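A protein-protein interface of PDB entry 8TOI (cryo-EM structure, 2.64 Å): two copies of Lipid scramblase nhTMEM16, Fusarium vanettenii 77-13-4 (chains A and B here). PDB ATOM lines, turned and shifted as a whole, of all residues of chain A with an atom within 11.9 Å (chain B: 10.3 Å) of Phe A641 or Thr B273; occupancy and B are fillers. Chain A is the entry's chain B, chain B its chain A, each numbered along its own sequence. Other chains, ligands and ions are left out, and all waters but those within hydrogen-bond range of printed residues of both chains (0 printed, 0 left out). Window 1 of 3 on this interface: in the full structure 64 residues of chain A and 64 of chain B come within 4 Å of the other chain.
Phe A641 touches just these residues of chain B: Thr B273 and Glu B275.
Of chain A, only Lys A638 (3.8 Å) and Phe A641 (3.6 Å) come within 4 Å of Thr B273.
Lys A638 touches just these residues of chain B: Ile B272 (3.1 Å) and Thr B273 (3.8 Å).
Arg A640 touches none of the printed residues of chain B.
No residue of chain B comes within 4 Å of Gln A642.
No residue of chain A comes within 4 Å of Asp B270.
No residue of chain A comes within 4 Å of Pro B271.
Gly B274 touches none of the printed residues of chain A.
Printed residues of chain B within 4 Å of Gln A634: Ile B272 (3.4 Å).
Of the printed residues of chain B, Arg A637 touches Ile B272.
Glu A636 touches none of the printed residues of chain B.
Glu B269 touches none of the printed residues of chain A.
The nearest residue of chain B that does not touch Phe A641 is Asp B270 (5.0 Å).
The nearest residue of chain A that does not touch Thr B273 is Arg A637 (4.6 Å).
No position is printed for both chains.
Of the 6 pairs that touch across the chains among the printed residues, none has its exchanged pair printed and touching as well.
Gln A634 touches Ile B272 (NE2 to CG2, 3.4 Å).
Arg A637 touches Ile B272 (NH1 to CD1, 3.4 Å).
Lys A638 touches Thr B273.
Phe A641 touches Thr B273 (CD2 to CG2, 3.6 Å).
Phe A641 touches Glu B275.
The backbone carbonyl oxygen of Ile B272 sits at hydrogen-bond distance from the side-chain amino group of Lys A638, at 3.1 Å.
OG1 of Thr B273 sits at hydrogen-bond distance from OE1 of Glu B275, 2.5 Å away.
The side-chain amide nitrogen (NE2) of Gln A642 lies close to the side-chain amino group (NZ) of Lys A638 (3.3 Å).
The side-chain carboxylate of Asp A629 is in salt-bridge range of the guanidinium group of Arg A637.
N of Asp B270 lies within hydrogen-bond range of O of Glu B275, 3.1 Å away.
Hydrophobic or aromatic side chains of chain A within 4 Å of the printed part of chain B: Phe A641.
Printed residues of chain B that touch a printed residue of chain A: Ile B272, Thr B273 and Glu B275.
Among the printed residues, 6 pairs touch across the chains.
Among the printed residues, no Asp or Glu carboxylate lies within 4 Å of a Lys or Arg side-chain nitrogen of the other chain.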
ATOM      1  N   VAL A  95      -2.989  12.312  22.684  1.00  0.00           N
ATOM      2  CA  VAL A  95      -2.708  12.906  23.985  1.00  0.00           C
ATOM      3  C   VAL A  95      -3.597  14.117  24.254  1.00  0.00           C
ATOM      4  O   VAL A  95      -3.804  14.483  25.419  1.00  0.00           O
ATOM      5  CB  VAL A  95      -1.206  13.244  24.076  1.00  0.00           C
ATOM      6  CG1 VAL A  95      -0.846  14.448  23.207  1.00  0.00           C
ATOM      7  CG2 VAL A  95      -0.744  13.423  25.527  1.00  0.00           C
ATOM      8  N   ASP A 629      17.660  16.024  19.372  1.00  0.00           N
ATOM      9  CA  ASP A 629      16.442  16.730  19.791  1.00  0.00           C
ATOM     10  C   ASP A 629      15.408  16.774  18.659  1.00  0.00           C
ATOM     11  O   ASP A 629      15.150  17.813  18.046  1.00  0.00           O
ATOM     12  CB  ASP A 629      16.755  18.138  20.318  1.00  0.00           C
ATOM     13  CG  ASP A 629      15.592  18.748  21.074  1.00  0.00           C
ATOM     14  OD1 ASP A 629      15.324  18.306  22.212  1.00  0.00           O
ATOM     15  OD2 ASP A 629      14.944  19.669  20.534  1.00  0.00           O
ATOM     16  N   PRO A 631      11.927  16.754  16.620  1.00  0.00           N
ATOM     17  CA  PRO A 631      10.793  17.654  16.898  1.00  0.00           C
ATOM     18  C   PRO A 631       9.578  16.977  17.510  1.00  0.00           C
ATOM     19  O   PRO A 631       8.679  17.686  17.977  1.00  0.00           O
ATOM     20  CB  PRO A 631      10.461  18.239  15.518  1.00  0.00           C
ATOM     21  CG  PRO A 631      10.978  17.236  14.552  1.00  0.00           C
ATOM     22  CD  PRO A 631      12.221  16.683  15.177  1.00  0.00           C
ATOM     23  N   GLY A 632       9.512  15.643  17.515  1.00  0.00           N
ATOM     24  CA  GLY A 632       8.421  14.974  18.204  1.00  0.00           C
ATOM     25  C   GLY A 632       8.474  15.167  19.709  1.00  0.00           C
ATOM     26  O   GLY A 632       7.482  15.554  20.332  1.00  0.00           O
ATOM     27  N   LEU A 633       9.646  14.934  20.308  1.00  0.00           N
ATOM     28  CA  LEU A 633       9.810  15.162  21.741  1.00  0.00           C
ATOM     29  C   LEU A 633       9.766  16.646  22.080  1.00  0.00           C
ATOM     30  O   LEU A 633       9.335  17.019  23.175  1.00  0.00           O
ATOM     31  CB  LEU A 633      11.123  14.544  22.220  1.00  0.00           C
ATOM     32  CG  LEU A 633      11.286  14.330  23.726  1.00  0.00           C
ATOM     33  CD1 LEU A 633      10.452  13.148  24.195  1.00  0.00           C
ATOM     34  CD2 LEU A 633      12.751  14.130  24.080  1.00  0.00           C
ATOM     35  N   GLN A 634      10.197  17.499  21.146  1.00  0.00           N
ATOM     36  CA  GLN A 634      10.090  18.942  21.323  1.00  0.00           C
ATOM     37  C   GLN A 634       8.630  19.384  21.370  1.00  0.00           C
ATOM     38  O   GLN A 634       8.240  20.195  22.220  1.00  0.00           O
ATOM     39  CB  GLN A 634      10.847  19.631  20.188  1.00  0.00           C
ATOM     40  CG  GLN A 634      10.823  21.141  20.167  1.00  0.00           C
ATOM     41  CD  GLN A 634      11.621  21.688  18.997  1.00  0.00           C
ATOM     42  OE1 GLN A 634      11.938  20.957  18.059  1.00  0.00           O
ATOM     43  NE2 GLN A 634      11.972  22.964  19.059  1.00  0.00           N
ATOM     44  N   LYS A 635       7.801  18.820  20.487  1.00  0.00           N
ATOM     45  CA  LYS A 635       6.369  19.103  20.510  1.00  0.00           C
ATOM     46  C   LYS A 635       5.709  18.514  21.751  1.00  0.00           C
ATOM     47  O   LYS A 635       4.763  19.101  22.287  1.00  0.00           O
ATOM     48  CB  LYS A 635       5.709  18.561  19.245  1.00  0.00           C
ATOM     49  CG  LYS A 635       4.349  19.166  18.949  1.00  0.00           C
ATOM     50  CD  LYS A 635       4.010  19.062  17.472  1.00  0.00           C
ATOM     51  CE  LYS A 635       3.741  17.621  17.074  1.00  0.00           C
ATOM     52  NZ  LYS A 635       2.631  17.025  17.870  1.00  0.00           N
ATOM     53  N   GLU A 636       6.196  17.362  22.222  1.00  0.00           N
ATOM     54  CA  GLU A 636       5.679  16.782  23.461  1.00  0.00           C
ATOM     55  C   GLU A 636       6.006  17.654  24.669  1.00  0.00           C
ATOM     56  O   GLU A 636       5.170  17.814  25.564  1.00  0.00           O
ATOM     57  CB  GLU A 636       6.236  15.372  23.659  1.00  0.00           C
ATOM     58  CG  GLU A 636       5.634  14.322  22.739  1.00  0.00           C
ATOM     59  CD  GLU A 636       4.153  14.115  22.973  1.00  0.00           C
ATOM     60  OE1 GLU A 636       3.730  14.103  24.150  1.00  0.00           O
ATOM     61  OE2 GLU A 636       3.412  13.962  21.981  1.00  0.00           O
ATOM     62  N   ARG A 637       7.214  18.220  24.712  1.00  0.00           N
ATOM     63  CA  ARG A 637       7.584  19.138  25.787  1.00  0.00           C
ATOM     64  C   ARG A 637       6.768  20.427  25.731  1.00  0.00           C
ATOM     65  O   ARG A 637       6.325  20.927  26.779  1.00  0.00           O
ATOM     66  CB  ARG A 637       9.086  19.430  25.715  1.00  0.00           C
ATOM     67  CG  ARG A 637       9.530  20.770  26.282  1.00  0.00           C
ATOM     68  CD  ARG A 637      11.002  20.739  26.651  1.00  0.00           C
ATOM     69  NE  ARG A 637      11.790  20.009  25.664  1.00  0.00           N
ATOM     70  CZ  ARG A 637      12.408  20.571  24.636  1.00  0.00           C
ATOM     71  NH1 ARG A 637      12.370  21.878  24.436  1.00  0.00           N
ATOM     72  NH2 ARG A 637      13.086  19.803  23.788  1.00  0.00           N
ATOM     73  N   LYS A 638       6.537  20.954  24.523  1.00  0.00           N
ATOM     74  CA  LYS A 638       5.694  22.138  24.359  1.00  0.00           C
ATOM     75  C   LYS A 638       4.255  21.858  24.788  1.00  0.00           C
ATOM     76  O   LYS A 638       3.620  22.691  25.446  1.00  0.00           O
ATOM     77  CB  LYS A 638       5.755  22.616  22.905  1.00  0.00           C
ATOM     78  CG  LYS A 638       4.651  23.579  22.495  1.00  0.00           C
ATOM     79  CD  LYS A 638       4.857  24.945  23.125  1.00  0.00           C
ATOM     80  CE  LYS A 638       3.881  25.963  22.565  1.00  0.00           C
ATOM     81  NZ  LYS A 638       3.930  27.247  23.317  1.00  0.00           N
ATOM     82  N   GLU A 639       3.737  20.674  24.452  1.00  0.00           N
ATOM     83  CA  GLU A 639       2.398  20.263  24.857  1.00  0.00           C
ATOM     84  C   GLU A 639       2.303  20.039  26.363  1.00  0.00           C
ATOM     85  O   GLU A 639       1.259  20.341  26.952  1.00  0.00           O
ATOM     86  CB  GLU A 639       2.016  19.024  24.015  1.00  0.00           C
ATOM     87  CG  GLU A 639       0.625  18.321  24.149  1.00  0.00           C
ATOM     88  CD  GLU A 639       0.310  17.633  25.477  1.00  0.00           C
ATOM     89  OE1 GLU A 639       1.240  17.222  26.201  1.00  0.00           O
ATOM     90  OE2 GLU A 639      -0.892  17.474  25.777  1.00  0.00           O
ATOM     91  N   ARG A 640       3.356  19.511  26.991  1.00  0.00           N
ATOM     92  CA  ARG A 640       3.347  19.321  28.438  1.00  0.00           C
ATOM     93  C   ARG A 640       3.391  20.653  29.173  1.00  0.00           C
ATOM     94  O   ARG A 640       2.765  20.811  30.228  1.00  0.00           O
ATOM     95  CB  ARG A 640       4.519  18.435  28.860  1.00  0.00           C
ATOM     96  N   PHE A 641       4.137  21.623  28.637  1.00  0.00           N
ATOM     97  CA  PHE A 641       4.096  22.968  29.203  1.00  0.00           C
ATOM     98  C   PHE A 641       2.756  23.649  28.948  1.00  0.00           C
ATOM     99  O   PHE A 641       2.295  24.437  29.781  1.00  0.00           O
ATOM    100  CB  PHE A 641       5.232  23.819  28.641  1.00  0.00           C
ATOM    101  CG  PHE A 641       6.471  23.809  29.486  1.00  0.00           C
ATOM    102  CD1 PHE A 641       6.426  24.230  30.805  1.00  0.00           C
ATOM    103  CD2 PHE A 641       7.682  23.385  28.960  1.00  0.00           C
ATOM    104  CE1 PHE A 641       7.566  24.226  31.589  1.00  0.00           C
ATOM    105  CE2 PHE A 641       8.827  23.377  29.736  1.00  0.00           C
ATOM    106  CZ  PHE A 641       8.768  23.799  31.053  1.00  0.00           C
ATOM    107  N   GLN A 642       2.122  23.362  27.809  1.00  0.00           N
ATOM    108  CA  GLN A 642       0.852  24.002  27.483  1.00  0.00           C
ATOM    109  C   GLN A 642      -0.307  23.404  28.270  1.00  0.00           C
ATOM    110  O   GLN A 642      -1.288  24.103  28.548  1.00  0.00           O
ATOM    111  CB  GLN A 642       0.578  23.902  25.983  1.00  0.00           C
ATOM    112  CG  GLN A 642       1.220  25.010  25.163  1.00  0.00           C
ATOM    113  CD  GLN A 642       0.896  26.391  25.697  1.00  0.00           C
ATOM    114  OE1 GLN A 642      -0.270  26.745  25.871  1.00  0.00           O
ATOM    115  NE2 GLN A 642       1.931  27.181  25.965  1.00  0.00           N
ATOM    116  N   THR A 643      -0.218  22.124  28.638  1.00  0.00           N
ATOM    117  CA  THR A 643      -1.271  21.458  29.397  1.00  0.00           C
ATOM    118  C   THR A 643      -1.055  21.541  30.902  1.00  0.00           C
ATOM    119  O   THR A 643      -1.508  20.654  31.639  1.00  0.00           O
ATOM    120  CB  THR A 643      -1.400  19.999  28.957  1.00  0.00           C
ATOM    121  OG1 THR A 643      -0.097  19.421  28.820  1.00  0.00           O
ATOM    122  CG2 THR A 643      -2.141  19.910  27.635  1.00  0.00           C
ATOM    123  N   TRP B  89       1.970  14.383  38.455  1.00  0.00           N
ATOM    124  CA  TRP B  89       0.900  14.081  37.504  1.00  0.00           C
ATOM    125  C   TRP B  89       1.224  14.585  36.101  1.00  0.00           C
ATOM    126  O   TRP B  89       0.946  13.892  35.116  1.00  0.00           O
ATOM    127  CB  TRP B  89      -0.421  14.668  37.990  1.00  0.00           C
ATOM    128  CG  TRP B  89      -1.588  14.305  37.129  1.00  0.00           C
ATOM    129  CD1 TRP B  89      -2.392  13.217  37.261  1.00  0.00           C
ATOM    130  CD2 TRP B  89      -2.095  15.044  36.014  1.00  0.00           C
ATOM    131  NE1 TRP B  89      -3.362  13.221  36.291  1.00  0.00           N
ATOM    132  CE2 TRP B  89      -3.200  14.334  35.511  1.00  0.00           C
ATOM    133  CE3 TRP B  89      -1.716  16.234  35.387  1.00  0.00           C
ATOM    134  CZ2 TRP B  89      -3.930  14.773  34.413  1.00  0.00           C
ATOM    135  CZ3 TRP B  89      -2.440  16.668  34.298  1.00  0.00           C
ATOM    136  CH2 TRP B  89      -3.535  15.941  33.821  1.00  0.00           C
ATOM    137  N   LEU B  90       1.778  15.798  35.982  1.00  0.00           N
ATOM    138  CA  LEU B  90       2.183  16.274  34.657  1.00  0.00           C
ATOM    139  C   LEU B  90       3.362  15.491  34.090  1.00  0.00           C
ATOM    140  O   LEU B  90       3.480  15.364  32.866  1.00  0.00           O
ATOM    141  CB  LEU B  90       2.514  17.768  34.667  1.00  0.00           C
ATOM    142  CG  LEU B  90       1.429  18.857  34.655  1.00  0.00           C
ATOM    143  CD1 LEU B  90       0.637  19.019  35.937  1.00  0.00           C
ATOM    144  CD2 LEU B  90       2.079  20.176  34.264  1.00  0.00           C
ATOM    145  N   HIS B  91       4.234  14.956  34.937  1.00  0.00           N
ATOM    146  CA  HIS B  91       5.392  14.223  34.447  1.00  0.00           C
ATOM    147  C   HIS B  91       5.137  12.730  34.294  1.00  0.00           C
ATOM    148  O   HIS B  91       6.060  11.994  33.932  1.00  0.00           O
ATOM    149  CB  HIS B  91       6.590  14.454  35.367  1.00  0.00           C
ATOM    150  CG  HIS B  91       7.250  15.782  35.169  1.00  0.00           C
ATOM    151  ND1 HIS B  91       8.312  15.962  34.310  1.00  0.00           N
ATOM    152  CD2 HIS B  91       6.997  16.994  35.716  1.00  0.00           C
ATOM    153  CE1 HIS B  91       8.685  17.230  34.336  1.00  0.00           C
ATOM    154  NE2 HIS B  91       7.903  17.876  35.182  1.00  0.00           N
ATOM    155  N   GLU B 130       9.130  29.261  42.826  1.00  0.00           N
ATOM    156  CA  GLU B 130       8.292  28.065  42.894  1.00  0.00           C
ATOM    157  C   GLU B 130       7.867  27.738  44.322  1.00  0.00           C
ATOM    158  O   GLU B 130       7.595  26.573  44.625  1.00  0.00           O
ATOM    159  CB  GLU B 130       8.955  26.825  42.273  1.00  0.00           C
ATOM    160  CG  GLU B 130       9.165  26.859  40.764  1.00  0.00           C
ATOM    161  CD  GLU B 130      10.416  27.591  40.351  1.00  0.00           C
ATOM    162  OE1 GLU B 130      11.168  28.018  41.246  1.00  0.00           O
ATOM    163  OE2 GLU B 130      10.637  27.747  39.132  1.00  0.00           O
ATOM    164  N   SER B 254      12.817  11.294  34.424  1.00  0.00           N
ATOM    165  CA  SER B 254      12.485  12.288  33.413  1.00  0.00           C
ATOM    166  C   SER B 254      12.343  13.684  34.001  1.00  0.00           C
ATOM    167  O   SER B 254      12.448  14.666  33.259  1.00  0.00           O
ATOM    168  CB  SER B 254      11.193  11.896  32.697  1.00  0.00           C
ATOM    169  OG  SER B 254      11.204  10.523  32.349  1.00  0.00           O
ATOM    170  N   GLN B 256      13.728  16.661  35.340  1.00  0.00           N
ATOM    171  CA  GLN B 256      15.042  17.283  35.436  1.00  0.00           C
ATOM    172  C   GLN B 256      15.084  18.204  36.645  1.00  0.00           C
ATOM    173  O   GLN B 256      14.245  19.099  36.782  1.00  0.00           O
ATOM    174  CB  GLN B 256      15.353  18.058  34.159  1.00  0.00           C
ATOM    175  CG  GLN B 256      15.264  17.229  32.893  1.00  0.00           C
ATOM    176  CD  GLN B 256      16.591  16.614  32.509  1.00  0.00           C
ATOM    177  OE1 GLN B 256      17.018  15.617  33.091  1.00  0.00           O
ATOM    178  NE2 GLN B 256      17.255  17.208  31.524  1.00  0.00           N
ATOM    179  N   ALA B 268      18.939  32.759  28.466  1.00  0.00           N
ATOM    180  CA  ALA B 268      18.217  32.854  27.211  1.00  0.00           C
ATOM    181  C   ALA B 268      16.773  32.409  27.413  1.00  0.00           C
ATOM    182  O   ALA B 268      16.360  32.029  28.509  1.00  0.00           O
ATOM    183  CB  ALA B 268      18.908  32.023  26.132  1.00  0.00           C
ATOM    184  N   GLU B 269      15.989  32.455  26.343  1.00  0.00           N
ATOM    185  CA  GLU B 269      14.606  32.013  26.374  1.00  0.00           C
ATOM    186  C   GLU B 269      14.480  30.663  25.684  1.00  0.00           C
ATOM    187  O   GLU B 269      15.250  30.336  24.776  1.00  0.00           O
ATOM    188  CB  GLU B 269      13.682  33.033  25.702  1.00  0.00           C
ATOM    189  CG  GLU B 269      14.088  33.406  24.285  1.00  0.00           C
ATOM    190  CD  GLU B 269      13.355  34.630  23.774  1.00  0.00           C
ATOM    191  OE1 GLU B 269      12.310  34.985  24.359  1.00  0.00           O
ATOM    192  OE2 GLU B 269      13.822  35.236  22.787  1.00  0.00           O
ATOM    193  N   ASP B 270      13.521  29.869  26.146  1.00  0.00           N
ATOM    194  CA  ASP B 270      13.223  28.610  25.483  1.00  0.00           C
ATOM    195  C   ASP B 270      12.600  28.886  24.116  1.00  0.00           C
ATOM    196  O   ASP B 270      11.742  29.765  23.991  1.00  0.00           O
ATOM    197  CB  ASP B 270      12.287  27.752  26.336  1.00  0.00           C
ATOM    198  CG  ASP B 270      12.976  27.180  27.560  1.00  0.00           C
ATOM    199  OD1 ASP B 270      14.223  27.203  27.607  1.00  0.00           O
ATOM    200  OD2 ASP B 270      12.351  26.687  28.523  1.00  0.00           O
ATOM    201  N   PRO B 271      13.016  28.162  23.073  1.00  0.00           N
ATOM    202  CA  PRO B 271      12.570  28.505  21.712  1.00  0.00           C
ATOM    203  C   PRO B 271      11.128  28.131  21.410  1.00  0.00           C
ATOM    204  O   PRO B 271      10.606  28.571  20.377  1.00  0.00           O
ATOM    205  CB  PRO B 271      13.538  27.718  20.812  1.00  0.00           C
ATOM    206  CG  PRO B 271      14.597  27.160  21.728  1.00  0.00           C
ATOM    207  CD  PRO B 271      13.967  27.042  23.072  1.00  0.00           C
ATOM    208  N   ILE B 272      10.466  27.346  22.258  1.00  0.00           N
ATOM    209  CA  ILE B 272       9.112  26.896  21.959  1.00  0.00           C
ATOM    210  C   ILE B 272       8.122  27.337  23.029  1.00  0.00           C
ATOM    211  O   ILE B 272       6.938  27.540  22.741  1.00  0.00           O
ATOM    212  CB  ILE B 272       9.071  25.368  21.785  1.00  0.00           C
ATOM    213  CG1 ILE B 272       9.832  24.679  22.921  1.00  0.00           C
ATOM    214  CG2 ILE B 272       9.627  24.979  20.433  1.00  0.00           C
ATOM    215  CD1 ILE B 272       9.522  23.213  23.056  1.00  0.00           C
ATOM    216  N   THR B 273       8.592  27.496  24.263  1.00  0.00           N
ATOM    217  CA  THR B 273       7.703  27.770  25.387  1.00  0.00           C
ATOM    218  C   THR B 273       7.932  29.129  26.027  1.00  0.00           C
ATOM    219  O   THR B 273       6.965  29.840  26.308  1.00  0.00           O
ATOM    220  CB  THR B 273       7.843  26.678  26.451  1.00  0.00           C
ATOM    221  OG1 THR B 273       9.189  26.653  26.942  1.00  0.00           O
ATOM    222  CG2 THR B 273       7.495  25.315  25.872  1.00  0.00           C
ATOM    223  N   GLY B 274       9.181  29.514  26.268  1.00  0.00           N
ATOM    224  CA  GLY B 274       9.491  30.853  26.722  1.00  0.00           C
ATOM    225  C   GLY B 274       9.925  31.001  28.165  1.00  0.00           C
ATOM    226  O   GLY B 274      10.070  32.140  28.627  1.00  0.00           O
ATOM    227  N   GLU B 275      10.121  29.909  28.898  1.00  0.00           N
ATOM    228  CA  GLU B 275      10.704  30.025  30.227  1.00  0.00           C
ATOM    229  C   GLU B 275      12.181  30.390  30.107  1.00  0.00           C
ATOM    230  O   GLU B 275      12.871  29.893  29.211  1.00  0.00           O
ATOM    231  CB  GLU B 275      10.546  28.724  31.018  1.00  0.00           C
ATOM    232  CG  GLU B 275       9.114  28.388  31.387  1.00  0.00           C
ATOM    233  CD  GLU B 275       8.442  27.527  30.346  1.00  0.00           C
ATOM    234  OE1 GLU B 275       9.150  27.064  29.431  1.00  0.00           O
ATOM    235  OE2 GLU B 275       7.213  27.325  30.436  1.00  0.00           O
ATOM    236  N   PRO B 276      12.695  31.261  30.978  1.00  0.00           N
ATOM    237  CA  PRO B 276      14.110  31.654  30.873  1.00  0.00           C
ATOM    238  C   PRO B 276      15.013  30.538  31.375  1.00  0.00           C
ATOM    239  O   PRO B 276      14.973  30.166  32.549  1.00  0.00           O
ATOM    240  CB  PRO B 276      14.206  32.907  31.752  1.00  0.00           C
ATOM    241  CG  PRO B 276      12.932  32.990  32.524  1.00  0.00           C
ATOM    242  CD  PRO B 276      12.034  31.860  32.149  1.00  0.00           C
ATOM    243  N   VAL B 277      15.828  30.004  30.471  1.00  0.00           N
ATOM    244  CA  VAL B 277      16.748  28.916  30.771  1.00  0.00           C
ATOM    245  C   VAL B 277      18.161  29.487  30.857  1.00  0.00           C
ATOM    246  O   VAL B 277      18.557  30.338  30.049  1.00  0.00           O
ATOM    247  CB  VAL B 277      16.621  27.769  29.744  1.00  0.00           C
ATOM    248  CG1 VAL B 277      16.939  28.212  28.313  1.00  0.00           C
ATOM    249  CG2 VAL B 277      17.477  26.573  30.145  1.00  0.00           C
